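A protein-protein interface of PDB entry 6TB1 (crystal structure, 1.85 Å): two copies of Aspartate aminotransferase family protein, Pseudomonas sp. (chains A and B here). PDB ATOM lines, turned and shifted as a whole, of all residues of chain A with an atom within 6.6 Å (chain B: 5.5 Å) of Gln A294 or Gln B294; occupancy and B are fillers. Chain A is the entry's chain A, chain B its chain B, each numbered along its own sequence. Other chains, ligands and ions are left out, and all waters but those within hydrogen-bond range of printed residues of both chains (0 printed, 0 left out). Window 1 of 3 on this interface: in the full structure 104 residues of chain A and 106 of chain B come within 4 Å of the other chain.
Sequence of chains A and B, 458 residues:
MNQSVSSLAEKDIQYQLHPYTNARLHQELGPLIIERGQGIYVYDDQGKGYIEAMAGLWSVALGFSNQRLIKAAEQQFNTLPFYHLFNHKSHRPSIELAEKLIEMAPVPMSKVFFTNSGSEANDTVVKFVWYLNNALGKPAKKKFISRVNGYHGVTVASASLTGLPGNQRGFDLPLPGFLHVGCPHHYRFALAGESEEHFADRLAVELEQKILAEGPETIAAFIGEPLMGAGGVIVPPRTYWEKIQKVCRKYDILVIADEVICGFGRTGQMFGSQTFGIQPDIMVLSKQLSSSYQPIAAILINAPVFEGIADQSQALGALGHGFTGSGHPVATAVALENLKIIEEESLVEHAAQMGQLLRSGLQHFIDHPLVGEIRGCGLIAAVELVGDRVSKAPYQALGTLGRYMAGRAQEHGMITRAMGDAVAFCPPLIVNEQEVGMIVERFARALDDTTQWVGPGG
NE2 of His A328 is in hydrogen-bond range of O of Ser B292, 2.9 Å away. The backbone carbonyl oxygen (O) of Tyr A293 is in hydrogen-bond range of a ring nitrogen (NE2) of His B328 (3.3 Å). NE2 of His A328 sits close to O of Tyr B293, at 3.3 Å. A ring nitrogen (NE2) of His B328 lies within hydrogen-bond range of the backbone carbonyl oxygen (O) of Ser A292 (2.9 Å). OE1 of Gln B294 lies within hydrogen-bond range of NE2 of Gln A294.
The side-chain hydroxyl of Ser A290 is in hydrogen-bond range of the backbone carbonyl oxygen of Gln A294, 2.7 Å away. The backbone carbonyl oxygen of Lys A287 sits at hydrogen-bond distance from the backbone NH of Ser A292, 3.2 Å away. O of Gln B294 lies within hydrogen-bond range of OG of Ser B290 (2.7 Å). ND1 of His A328 is in hydrogen-bond range of N of Val A330 (3.1 Å). The backbone carbonyl oxygen (O) of His A328 sits at hydrogen-bond distance from the side-chain hydroxyl (OG1) of Thr A332, 2.9 Å away. OG of Ser A290 lies close to N of Ser A292.
Phe B77 touches Ala A73. Phe A77 touches Tyr B293 (CE1 to O, 3.6 Å). Phe A77 touches Gln B294. Pro A81 touches Tyr B293. Ser B292 touches Phe A82. CB of Pro B295 touches OD1 of Asn A116 (3.6 Å). O of Tyr A293 touches CE1 of Phe B77, 3.6 Å away. Gln A294 touches Phe B77.
Of the printed residues of chain B, Phe A77 touches Tyr B293 and Gln B294. Printed residues of chain B within 4 Å of Phe A82: Ser B292. Of the printed residues of chain B, Asn A116 touches Pro B295 (3.6 Å). Gln A294 touches two residues of chain B. Ile A296 touches none of the printed residues of chain B. Of the printed residues of chain A, Phe B77 touches Ala A73 (3.5 Å), Tyr A293 (3.6 Å) and Gln A294 (3.7 Å). Of the printed residues of chain A, Gln B294 touches Phe A77 (3.7 Å) and Gln A294 (2.9 Å). Of the printed residues of chain A, Pro B295 touches Asn A116 (3.6 Å). Val B330 touches none of the printed residues of chain A. The nearest residue of chain B that does not touch Gln A294 is His B328 (4.03 Å).
Printed residues of chain B that touch a printed residue of chain A: Phe B77, Ser B292, Tyr B293, Gln B294, Pro B295 and His B328. Hydrophobic or aromatic side chains of chain B within 4 Å of the printed part of chain A: Phe B77, Tyr B293, Pro B295 and His B328. Printed residues of chain A that touch a printed residue of chain B: Ala A73, Phe A77, Pro A81, Phe A82, Asn A116, Ser A292, Tyr A293, Gln A294 and His A328. Hydrophobic or aromatic side chains of chain A within 4 Å of the printed part of chain B: Ala A73, Phe A77, Pro A81, Phe A82 and His A328. Among the printed residues, 13 pairs touch across the chains. Among the printed residues, no Asp or Glu carboxylate lies within 4 Å of a Lys or Arg side-chain nitrogen of the other chain.
Phe A77 touches Tyr B293, and with the chains exchanged Tyr A293 touches Phe B77. Phe A77 touches Gln B294, and with the chains exchanged Gln A294 touches Phe B77. Ser A292 touches His B328, and with the chains exchanged His A328 touches Ser B292. Gln B294 touches its own counterpart, Gln A294. 11 positions are printed for both chains. Of the 13 pairs that touch across the chains among the printed residues, 9 have their exchanged pair printed and touching as well.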
ATOM      1  N   ALA A  73     -26.955 -15.498 -10.143  1.00  0.00           N
ATOM      2  CA  ALA A  73     -25.841 -14.521 -10.216  1.00  0.00           C
ATOM      3  C   ALA A  73     -24.522 -15.243 -10.513  1.00  0.00           C
ATOM      4  O   ALA A  73     -23.820 -14.840 -11.449  1.00  0.00           O
ATOM      5  CB  ALA A  73     -25.746 -13.734  -8.935  1.00  0.00           C
ATOM      6  N   PHE A  77     -22.085 -14.712 -13.723  1.00  0.00           N
ATOM      7  CA  PHE A  77     -20.706 -14.209 -13.463  1.00  0.00           C
ATOM      8  C   PHE A  77     -19.684 -15.085 -14.208  1.00  0.00           C
ATOM      9  O   PHE A  77     -18.731 -14.559 -14.830  1.00  0.00           O
ATOM     10  CB  PHE A  77     -20.374 -14.181 -11.970  1.00  0.00           C
ATOM     11  CG  PHE A  77     -20.742 -12.920 -11.219  1.00  0.00           C
ATOM     12  CD1 PHE A  77     -20.302 -11.668 -11.640  1.00  0.00           C
ATOM     13  CD2 PHE A  77     -21.510 -12.988 -10.066  1.00  0.00           C
ATOM     14  CE1 PHE A  77     -20.654 -10.523 -10.939  1.00  0.00           C
ATOM     15  CE2 PHE A  77     -21.839 -11.838  -9.354  1.00  0.00           C
ATOM     16  CZ  PHE A  77     -21.401 -10.608  -9.792  1.00  0.00           C
ATOM     17  N   PRO A  81     -19.585 -11.682 -17.110  1.00  0.00           N
ATOM     18  CA  PRO A  81     -19.885 -10.868 -15.932  1.00  0.00           C
ATOM     19  C   PRO A  81     -20.240  -9.403 -16.244  1.00  0.00           C
ATOM     20  O   PRO A  81     -20.880  -8.764 -15.419  1.00  0.00           O
ATOM     21  CB  PRO A  81     -18.600 -10.998 -15.100  1.00  0.00           C
ATOM     22  CG  PRO A  81     -17.501 -11.172 -16.140  1.00  0.00           C
ATOM     23  CD  PRO A  81     -18.148 -11.959 -17.262  1.00  0.00           C
ATOM     24  N   PHE A  82     -19.849  -8.903 -17.416  1.00  0.00           N
ATOM     25  CA  PHE A  82     -20.303  -7.588 -17.944  1.00  0.00           C
ATOM     26  C   PHE A  82     -20.348  -7.660 -19.463  1.00  0.00           C
ATOM     27  O   PHE A  82     -19.415  -8.212 -20.097  1.00  0.00           O
ATOM     28  CB  PHE A  82     -19.409  -6.421 -17.505  1.00  0.00           C
ATOM     29  CG  PHE A  82     -19.802  -5.105 -18.142  1.00  0.00           C
ATOM     30  CD1 PHE A  82     -20.885  -4.384 -17.665  1.00  0.00           C
ATOM     31  CD2 PHE A  82     -19.158  -4.640 -19.276  1.00  0.00           C
ATOM     32  CE1 PHE A  82     -21.286  -3.197 -18.278  1.00  0.00           C
ATOM     33  CE2 PHE A  82     -19.554  -3.454 -19.885  1.00  0.00           C
ATOM     34  CZ  PHE A  82     -20.613  -2.732 -19.376  1.00  0.00           C
ATOM     35  N   ASN A 116     -30.450   1.448 -14.233  1.00  0.00           N
ATOM     36  CA  ASN A 116     -30.028   0.918 -12.907  1.00  0.00           C
ATOM     37  C   ASN A 116     -31.090   1.220 -11.859  1.00  0.00           C
ATOM     38  O   ASN A 116     -31.329   0.342 -11.007  1.00  0.00           O
ATOM     39  CB  ASN A 116     -28.676   1.461 -12.459  1.00  0.00           C
ATOM     40  CG  ASN A 116     -27.608   1.311 -13.519  1.00  0.00           C
ATOM     41  OD1 ASN A 116     -27.188   0.200 -13.831  1.00  0.00           O
ATOM     42  ND2 ASN A 116     -27.195   2.432 -14.096  1.00  0.00           N
ATOM     43  N   SER A 286     -39.118  -1.320 -10.785  1.00  0.00           N
ATOM     44  CA  SER A 286     -37.813  -1.506 -10.088  1.00  0.00           C
ATOM     45  C   SER A 286     -38.060  -2.299  -8.803  1.00  0.00           C
ATOM     46  O   SER A 286     -39.071  -3.011  -8.729  1.00  0.00           O
ATOM     47  CB  SER A 286     -37.112  -0.174  -9.824  1.00  0.00           C
ATOM     48  OG  SER A 286     -35.729  -0.370  -9.498  1.00  0.00           O
ATOM     49  N   LYS A 287     -37.159  -2.182  -7.823  1.00  0.00           N
ATOM     50  CA  LYS A 287     -37.341  -2.689  -6.437  1.00  0.00           C
ATOM     51  C   LYS A 287     -37.688  -4.192  -6.464  1.00  0.00           C
ATOM     52  O   LYS A 287     -36.746  -4.999  -6.580  1.00  0.00           O
ATOM     53  CB  LYS A 287     -38.340  -1.784  -5.702  1.00  0.00           C
ATOM     54  CG  LYS A 287     -37.749  -0.464  -5.177  1.00  0.00           C
ATOM     55  CD  LYS A 287     -38.712   0.398  -4.313  1.00  0.00           C
ATOM     56  CE  LYS A 287     -38.090   1.653  -3.680  1.00  0.00           C
ATOM     57  NZ  LYS A 287     -38.499   2.944  -4.313  1.00  0.00           N
ATOM     58  N   SER A 290     -36.101  -7.258  -8.790  1.00  0.00           N
ATOM     59  CA  SER A 290     -34.911  -8.085  -8.488  1.00  0.00           C
ATOM     60  C   SER A 290     -34.838  -8.462  -6.999  1.00  0.00           C
ATOM     61  O   SER A 290     -33.781  -8.989  -6.585  1.00  0.00           O
ATOM     62  CB  SER A 290     -33.638  -7.402  -8.947  1.00  0.00           C
ATOM     63  OG  SER A 290     -33.383  -6.247  -8.162  1.00  0.00           O
ATOM     64  N   SER A 291     -35.876  -8.187  -6.211  1.00  0.00           N
ATOM     65  CA  SER A 291     -35.836  -8.222  -4.725  1.00  0.00           C
ATOM     66  C   SER A 291     -34.694  -7.330  -4.215  1.00  0.00           C
ATOM     67  O   SER A 291     -34.188  -7.567  -3.097  1.00  0.00           O
ATOM     68  CB  SER A 291     -35.731  -9.661  -4.200  1.00  0.00           C
ATOM     69  OG  SER A 291     -36.958 -10.374  -4.343  1.00  0.00           O
ATOM     70  N   SER A 292     -34.311  -6.319  -4.995  1.00  0.00           N
ATOM     71  CA  SER A 292     -33.138  -5.429  -4.758  1.00  0.00           C
ATOM     72  C   SER A 292     -31.820  -6.212  -4.601  1.00  0.00           C
ATOM     73  O   SER A 292     -30.856  -5.594  -4.129  1.00  0.00           O
ATOM     74  CB  SER A 292     -33.361  -4.527  -3.554  1.00  0.00           C
ATOM     75  OG  SER A 292     -34.280  -3.507  -3.846  1.00  0.00           O
ATOM     76  N   TYR A 293     -31.722  -7.476  -5.034  1.00  0.00           N
ATOM     77  CA  TYR A 293     -30.447  -8.253  -4.962  1.00  0.00           C
ATOM     78  C   TYR A 293     -29.434  -7.670  -5.951  1.00  0.00           C
ATOM     79  O   TYR A 293     -28.208  -7.823  -5.735  1.00  0.00           O
ATOM     80  CB  TYR A 293     -30.664  -9.745  -5.247  1.00  0.00           C
ATOM     81  CG  TYR A 293     -31.048 -10.596  -4.058  1.00  0.00           C
ATOM     82  CD1 TYR A 293     -32.050 -10.197  -3.184  1.00  0.00           C
ATOM     83  CD2 TYR A 293     -30.486 -11.851  -3.856  1.00  0.00           C
ATOM     84  CE1 TYR A 293     -32.436 -10.981  -2.107  1.00  0.00           C
ATOM     85  CE2 TYR A 293     -30.882 -12.659  -2.795  1.00  0.00           C
ATOM     86  CZ  TYR A 293     -31.853 -12.224  -1.910  1.00  0.00           C
ATOM     87  OH  TYR A 293     -32.270 -13.002  -0.856  1.00  0.00           O
ATOM     88  N   GLN A 294     -29.934  -6.989  -6.990  1.00  0.00           N
ATOM     89  CA  GLN A 294     -29.135  -6.225  -7.979  1.00  0.00           C
ATOM     90  C   GLN A 294     -29.832  -4.903  -8.310  1.00  0.00           C
ATOM     91  O   GLN A 294     -31.062  -4.839  -8.340  1.00  0.00           O
ATOM     92  CB  GLN A 294     -28.955  -7.052  -9.254  1.00  0.00           C
ATOM     93  CG  GLN A 294     -28.080  -8.286  -9.057  1.00  0.00           C
ATOM     94  CD  GLN A 294     -26.621  -7.938  -8.971  1.00  0.00           C
ATOM     95  OE1 GLN A 294     -25.955  -7.776  -9.986  1.00  0.00           O
ATOM     96  NE2 GLN A 294     -26.116  -7.801  -7.754  1.00  0.00           N
ATOM     97  N   PRO A 295     -29.086  -3.795  -8.556  1.00  0.00           N
ATOM     98  CA  PRO A 295     -29.693  -2.538  -9.008  1.00  0.00           C
ATOM     99  C   PRO A 295     -30.168  -2.663 -10.462  1.00  0.00           C
ATOM    100  O   PRO A 295     -29.349  -2.836 -11.343  1.00  0.00           O
ATOM    101  CB  PRO A 295     -28.566  -1.498  -8.908  1.00  0.00           C
ATOM    102  CG  PRO A 295     -27.512  -2.161  -8.067  1.00  0.00           C
ATOM    103  CD  PRO A 295     -27.642  -3.648  -8.326  1.00  0.00           C
ATOM    104  N   ILE A 296     -31.486  -2.644 -10.670  1.00  0.00           N
ATOM    105  CA  ILE A 296     -32.086  -2.655 -12.035  1.00  0.00           C
ATOM    106  C   ILE A 296     -33.482  -2.035 -11.998  1.00  0.00           C
ATOM    107  O   ILE A 296     -34.218  -2.200 -10.977  1.00  0.00           O
ATOM    108  CB  ILE A 296     -32.100  -4.081 -12.628  1.00  0.00           C
ATOM    109  CG1 ILE A 296     -32.812  -4.131 -13.984  1.00  0.00           C
ATOM    110  CG2 ILE A 296     -32.719  -5.069 -11.644  1.00  0.00           C
ATOM    111  CD1 ILE A 296     -32.584  -5.440 -14.739  1.00  0.00           C
ATOM    112  N   ALA A 297     -33.822  -1.334 -13.081  1.00  0.00           N
ATOM    113  CA  ALA A 297     -35.173  -0.799 -13.354  1.00  0.00           C
ATOM    114  C   ALA A 297     -35.485  -1.000 -14.846  1.00  0.00           C
ATOM    115  O   ALA A 297     -34.537  -1.153 -15.657  1.00  0.00           O
ATOM    116  CB  ALA A 297     -35.260   0.661 -12.954  1.00  0.00           C
ATOM    117  N   HIS A 328     -27.535  -4.718 -17.536  1.00  0.00           N
ATOM    118  CA  HIS A 328     -26.346  -5.447 -17.018  1.00  0.00           C
ATOM    119  C   HIS A 328     -26.672  -6.939 -16.939  1.00  0.00           C
ATOM    120  O   HIS A 328     -27.683  -7.318 -16.355  1.00  0.00           O
ATOM    121  CB  HIS A 328     -25.953  -4.908 -15.623  1.00  0.00           C
ATOM    122  CG  HIS A 328     -24.644  -5.414 -15.125  1.00  0.00           C
ATOM    123  ND1 HIS A 328     -24.462  -6.736 -14.713  1.00  0.00           N
ATOM    124  CD2 HIS A 328     -23.451  -4.798 -14.965  1.00  0.00           C
ATOM    125  CE1 HIS A 328     -23.204  -6.904 -14.330  1.00  0.00           C
ATOM    126  NE2 HIS A 328     -22.563  -5.727 -14.447  1.00  0.00           N
ATOM    127  N   VAL A 330     -25.687  -9.560 -15.204  1.00  0.00           N
ATOM    128  CA  VAL A 330     -25.910 -10.161 -13.855  1.00  0.00           C
ATOM    129  C   VAL A 330     -27.231  -9.635 -13.273  1.00  0.00           C
ATOM    130  O   VAL A 330     -27.991 -10.447 -12.704  1.00  0.00           O
ATOM    131  CB  VAL A 330     -24.719  -9.956 -12.899  1.00  0.00           C
ATOM    132  CG1 VAL A 330     -24.962 -10.672 -11.583  1.00  0.00           C
ATOM    133  CG2 VAL A 330     -23.431 -10.465 -13.524  1.00  0.00           C
ATOM    134  N   ALA A 331     -27.523  -8.334 -13.412  1.00  0.00           N
ATOM    135  CA  ALA A 331     -28.764  -7.735 -12.860  1.00  0.00           C
ATOM    136  C   ALA A 331     -29.988  -8.315 -13.585  1.00  0.00           C
ATOM    137  O   ALA A 331     -31.011  -8.631 -12.898  1.00  0.00           O
ATOM    138  CB  ALA A 331     -28.722  -6.228 -12.936  1.00  0.00           C
ATOM    139  N   THR A 332     -29.917  -8.465 -14.909  1.00  0.00           N
ATOM    140  CA  THR A 332     -31.050  -9.010 -15.717  1.00  0.00           C
ATOM    141  C   THR A 332     -31.244 -10.509 -15.410  1.00  0.00           C
ATOM    142  O   THR A 332     -32.416 -10.943 -15.325  1.00  0.00           O
ATOM    143  CB  THR A 332     -30.886  -8.688 -17.209  1.00  0.00           C
ATOM    144  OG1 THR A 332     -29.600  -9.087 -17.695  1.00  0.00           O
ATOM    145  CG2 THR A 332     -31.089  -7.221 -17.501  1.00  0.00           C
ATOM    146  N   VAL A 334     -30.584 -12.104 -12.585  1.00  0.00           N
ATOM    147  CA  VAL A 334     -31.189 -12.199 -11.231  1.00  0.00           C
ATOM    148  C   VAL A 334     -32.665 -11.798 -11.308  1.00  0.00           C
ATOM    149  O   VAL A 334     -33.506 -12.489 -10.686  1.00  0.00           O
ATOM    150  CB  VAL A 334     -30.398 -11.356 -10.209  1.00  0.00           C
ATOM    151  CG1 VAL A 334     -31.175 -11.176  -8.912  1.00  0.00           C
ATOM    152  CG2 VAL A 334     -29.027 -11.989  -9.966  1.00  0.00           C
ATOM    153  N   ALA A 335     -33.007 -10.713 -12.006  1.00  0.00           N
ATOM    154  CA  ALA A 335     -34.418 -10.259 -12.107  1.00  0.00           C
ATOM    155  C   ALA A 335     -35.260 -11.355 -12.797  1.00  0.00           C
ATOM    156  O   ALA A 335     -36.383 -11.644 -12.332  1.00  0.00           O
ATOM    157  CB  ALA A 335     -34.505  -8.940 -12.841  1.00  0.00           C
ATOM    158  N   PHE B  77     -23.440 -12.074  -0.953  1.00  0.00           N
ATOM    159  CA  PHE B  77     -24.830 -12.555  -1.198  1.00  0.00           C
ATOM    160  C   PHE B  77     -25.283 -13.461  -0.041  1.00  0.00           C
ATOM    161  O   PHE B  77     -26.441 -13.355   0.441  1.00  0.00           O
ATOM    162  CB  PHE B  77     -24.947 -13.332  -2.514  1.00  0.00           C
ATOM    163  CG  PHE B  77     -25.220 -12.531  -3.767  1.00  0.00           C
ATOM    164  CD1 PHE B  77     -26.334 -11.715  -3.863  1.00  0.00           C
ATOM    165  CD2 PHE B  77     -24.396 -12.657  -4.883  1.00  0.00           C
ATOM    166  CE1 PHE B  77     -26.612 -11.022  -5.034  1.00  0.00           C
ATOM    167  CE2 PHE B  77     -24.674 -11.963  -6.052  1.00  0.00           C
ATOM    168  CZ  PHE B  77     -25.786 -11.154  -6.128  1.00  0.00           C
ATOM    169  N   SER B 290     -15.303  -1.066 -10.250  1.00  0.00           N
ATOM    170  CA  SER B 290     -15.779  -2.457 -10.037  1.00  0.00           C
ATOM    171  C   SER B 290     -15.430  -3.373 -11.216  1.00  0.00           C
ATOM    172  O   SER B 290     -15.957  -4.502 -11.251  1.00  0.00           O
ATOM    173  CB  SER B 290     -17.263  -2.482  -9.752  1.00  0.00           C
ATOM    174  OG  SER B 290     -18.009  -2.086 -10.908  1.00  0.00           O
ATOM    175  N   SER B 292     -16.755  -2.918 -13.844  1.00  0.00           N
ATOM    176  CA  SER B 292     -18.176  -3.013 -14.287  1.00  0.00           C
ATOM    177  C   SER B 292     -18.826  -4.360 -13.933  1.00  0.00           C
ATOM    178  O   SER B 292     -19.899  -4.644 -14.502  1.00  0.00           O
ATOM    179  CB  SER B 292     -18.311  -2.727 -15.770  1.00  0.00           C
ATOM    180  OG  SER B 292     -18.167  -1.344 -16.036  1.00  0.00           O
ATOM    181  N   TYR B 293     -18.269  -5.158 -13.006  1.00  0.00           N
ATOM    182  CA  TYR B 293     -18.896  -6.450 -12.589  1.00  0.00           C
ATOM    183  C   TYR B 293     -20.203  -6.170 -11.830  1.00  0.00           C
ATOM    184  O   TYR B 293     -21.119  -7.034 -11.803  1.00  0.00           O
ATOM    185  CB  TYR B 293     -17.947  -7.308 -11.750  1.00  0.00           C
ATOM    186  CG  TYR B 293     -17.019  -8.213 -12.531  1.00  0.00           C
ATOM    187  CD1 TYR B 293     -16.285  -7.739 -13.602  1.00  0.00           C
ATOM    188  CD2 TYR B 293     -16.766  -9.513 -12.110  1.00  0.00           C
ATOM    189  CE1 TYR B 293     -15.376  -8.537 -14.282  1.00  0.00           C
ATOM    190  CE2 TYR B 293     -15.862 -10.329 -12.781  1.00  0.00           C
ATOM    191  CZ  TYR B 293     -15.166  -9.843 -13.873  1.00  0.00           C
ATOM    192  OH  TYR B 293     -14.261 -10.630 -14.539  1.00  0.00           O
ATOM    193  N   GLN B 294     -20.295  -4.973 -11.238  1.00  0.00           N
ATOM    194  CA  GLN B 294     -21.510  -4.459 -10.546  1.00  0.00           C
ATOM    195  C   GLN B 294     -21.711  -2.979 -10.885  1.00  0.00           C
ATOM    196  O   GLN B 294     -20.737  -2.245 -11.002  1.00  0.00           O
ATOM    197  CB  GLN B 294     -21.333  -4.627  -9.033  1.00  0.00           C
ATOM    198  CG  GLN B 294     -21.356  -6.094  -8.582  1.00  0.00           C
ATOM    199  CD  GLN B 294     -22.757  -6.646  -8.609  1.00  0.00           C
ATOM    200  OE1 GLN B 294     -23.537  -6.445  -7.675  1.00  0.00           O
ATOM    201  NE2 GLN B 294     -23.085  -7.345  -9.689  1.00  0.00           N
ATOM    202  N   PRO B 295     -22.965  -2.486 -11.009  1.00  0.00           N
ATOM    203  CA  PRO B 295     -23.204  -1.055 -11.203  1.00  0.00           C
ATOM    204  C   PRO B 295     -22.925  -0.287  -9.902  1.00  0.00           C
ATOM    205  O   PRO B 295     -23.635  -0.467  -8.925  1.00  0.00           O
ATOM    206  CB  PRO B 295     -24.681  -0.944 -11.589  1.00  0.00           C
ATOM    207  CG  PRO B 295     -25.165  -2.385 -11.806  1.00  0.00           C
ATOM    208  CD  PRO B 295     -24.217  -3.268 -11.020  1.00  0.00           C
ATOM    209  N   ILE B 296     -21.879   0.534  -9.909  1.00  0.00           N
ATOM    210  CA  ILE B 296     -21.571   1.424  -8.749  1.00  0.00           C
ATOM    211  C   ILE B 296     -20.763   2.630  -9.237  1.00  0.00           C
ATOM    212  O   ILE B 296     -19.904   2.487 -10.146  1.00  0.00           O
ATOM    213  CB  ILE B 296     -20.839   0.639  -7.632  1.00  0.00           C
ATOM    214  CG1 ILE B 296     -20.415   1.545  -6.473  1.00  0.00           C
ATOM    215  CG2 ILE B 296     -19.649  -0.129  -8.194  1.00  0.00           C
ATOM    216  CD1 ILE B 296     -19.894   0.782  -5.259  1.00  0.00           C
ATOM    217  N   HIS B 328     -24.901  -0.263  -2.351  1.00  0.00           N
ATOM    218  CA  HIS B 328     -25.378  -1.672  -2.391  1.00  0.00           C
ATOM    219  C   HIS B 328     -24.273  -2.610  -1.886  1.00  0.00           C
ATOM    220  O   HIS B 328     -23.159  -2.576  -2.393  1.00  0.00           O
ATOM    221  CB  HIS B 328     -25.808  -2.065  -3.803  1.00  0.00           C
ATOM    222  CG  HIS B 328     -26.556  -3.362  -3.860  1.00  0.00           C
ATOM    223  ND1 HIS B 328     -25.929  -4.588  -3.681  1.00  0.00           N
ATOM    224  CD2 HIS B 328     -27.858  -3.631  -4.122  1.00  0.00           C
ATOM    225  CE1 HIS B 328     -26.834  -5.547  -3.787  1.00  0.00           C
ATOM    226  NE2 HIS B 328     -28.019  -4.992  -4.064  1.00  0.00           N
ATOM    227  N   VAL B 330     -23.433  -5.812  -2.198  1.00  0.00           N
ATOM    228  CA  VAL B 330     -22.743  -6.682  -3.196  1.00  0.00           C
ATOM    229  C   VAL B 330     -21.860  -5.811  -4.107  1.00  0.00           C
ATOM    230  O   VAL B 330     -20.708  -6.220  -4.395  1.00  0.00           O
ATOM    231  CB  VAL B 330     -23.730  -7.556  -3.986  1.00  0.00           C
ATOM    232  CG1 VAL B 330     -22.998  -8.479  -4.961  1.00  0.00           C
ATOM    233  CG2 VAL B 330     -24.610  -8.372  -3.046  1.00  0.00           C
ATOM    234  N   ALA B 331     -22.336  -4.647  -4.559  1.00  0.00           N
ATOM    235  CA  ALA B 331     -21.564  -3.769  -5.479  1.00  0.00           C
ATOM    236  C   ALA B 331     -20.333  -3.211  -4.748  1.00  0.00           C
ATOM    237  O   ALA B 331     -19.251  -3.164  -5.353  1.00  0.00           O
ATOM    238  CB  ALA B 331     -22.455  -2.658  -6.017  1.00  0.00           C
ATOM    239  N   VAL B 334     -17.671  -6.044  -4.151  1.00  0.00           N
ATOM    240  CA  VAL B 334     -16.937  -6.360  -5.414  1.00  0.00           C
ATOM    241  C   VAL B 334     -15.937  -5.236  -5.706  1.00  0.00           C
ATOM    242  O   VAL B 334     -14.788  -5.541  -6.064  1.00  0.00           O
ATOM    243  CB  VAL B 334     -17.926  -6.599  -6.565  1.00  0.00           C
ATOM    244  CG1 VAL B 334     -17.265  -6.574  -7.932  1.00  0.00           C
ATOM    245  CG2 VAL B 334     -18.670  -7.902  -6.353  1.00  0.00           C
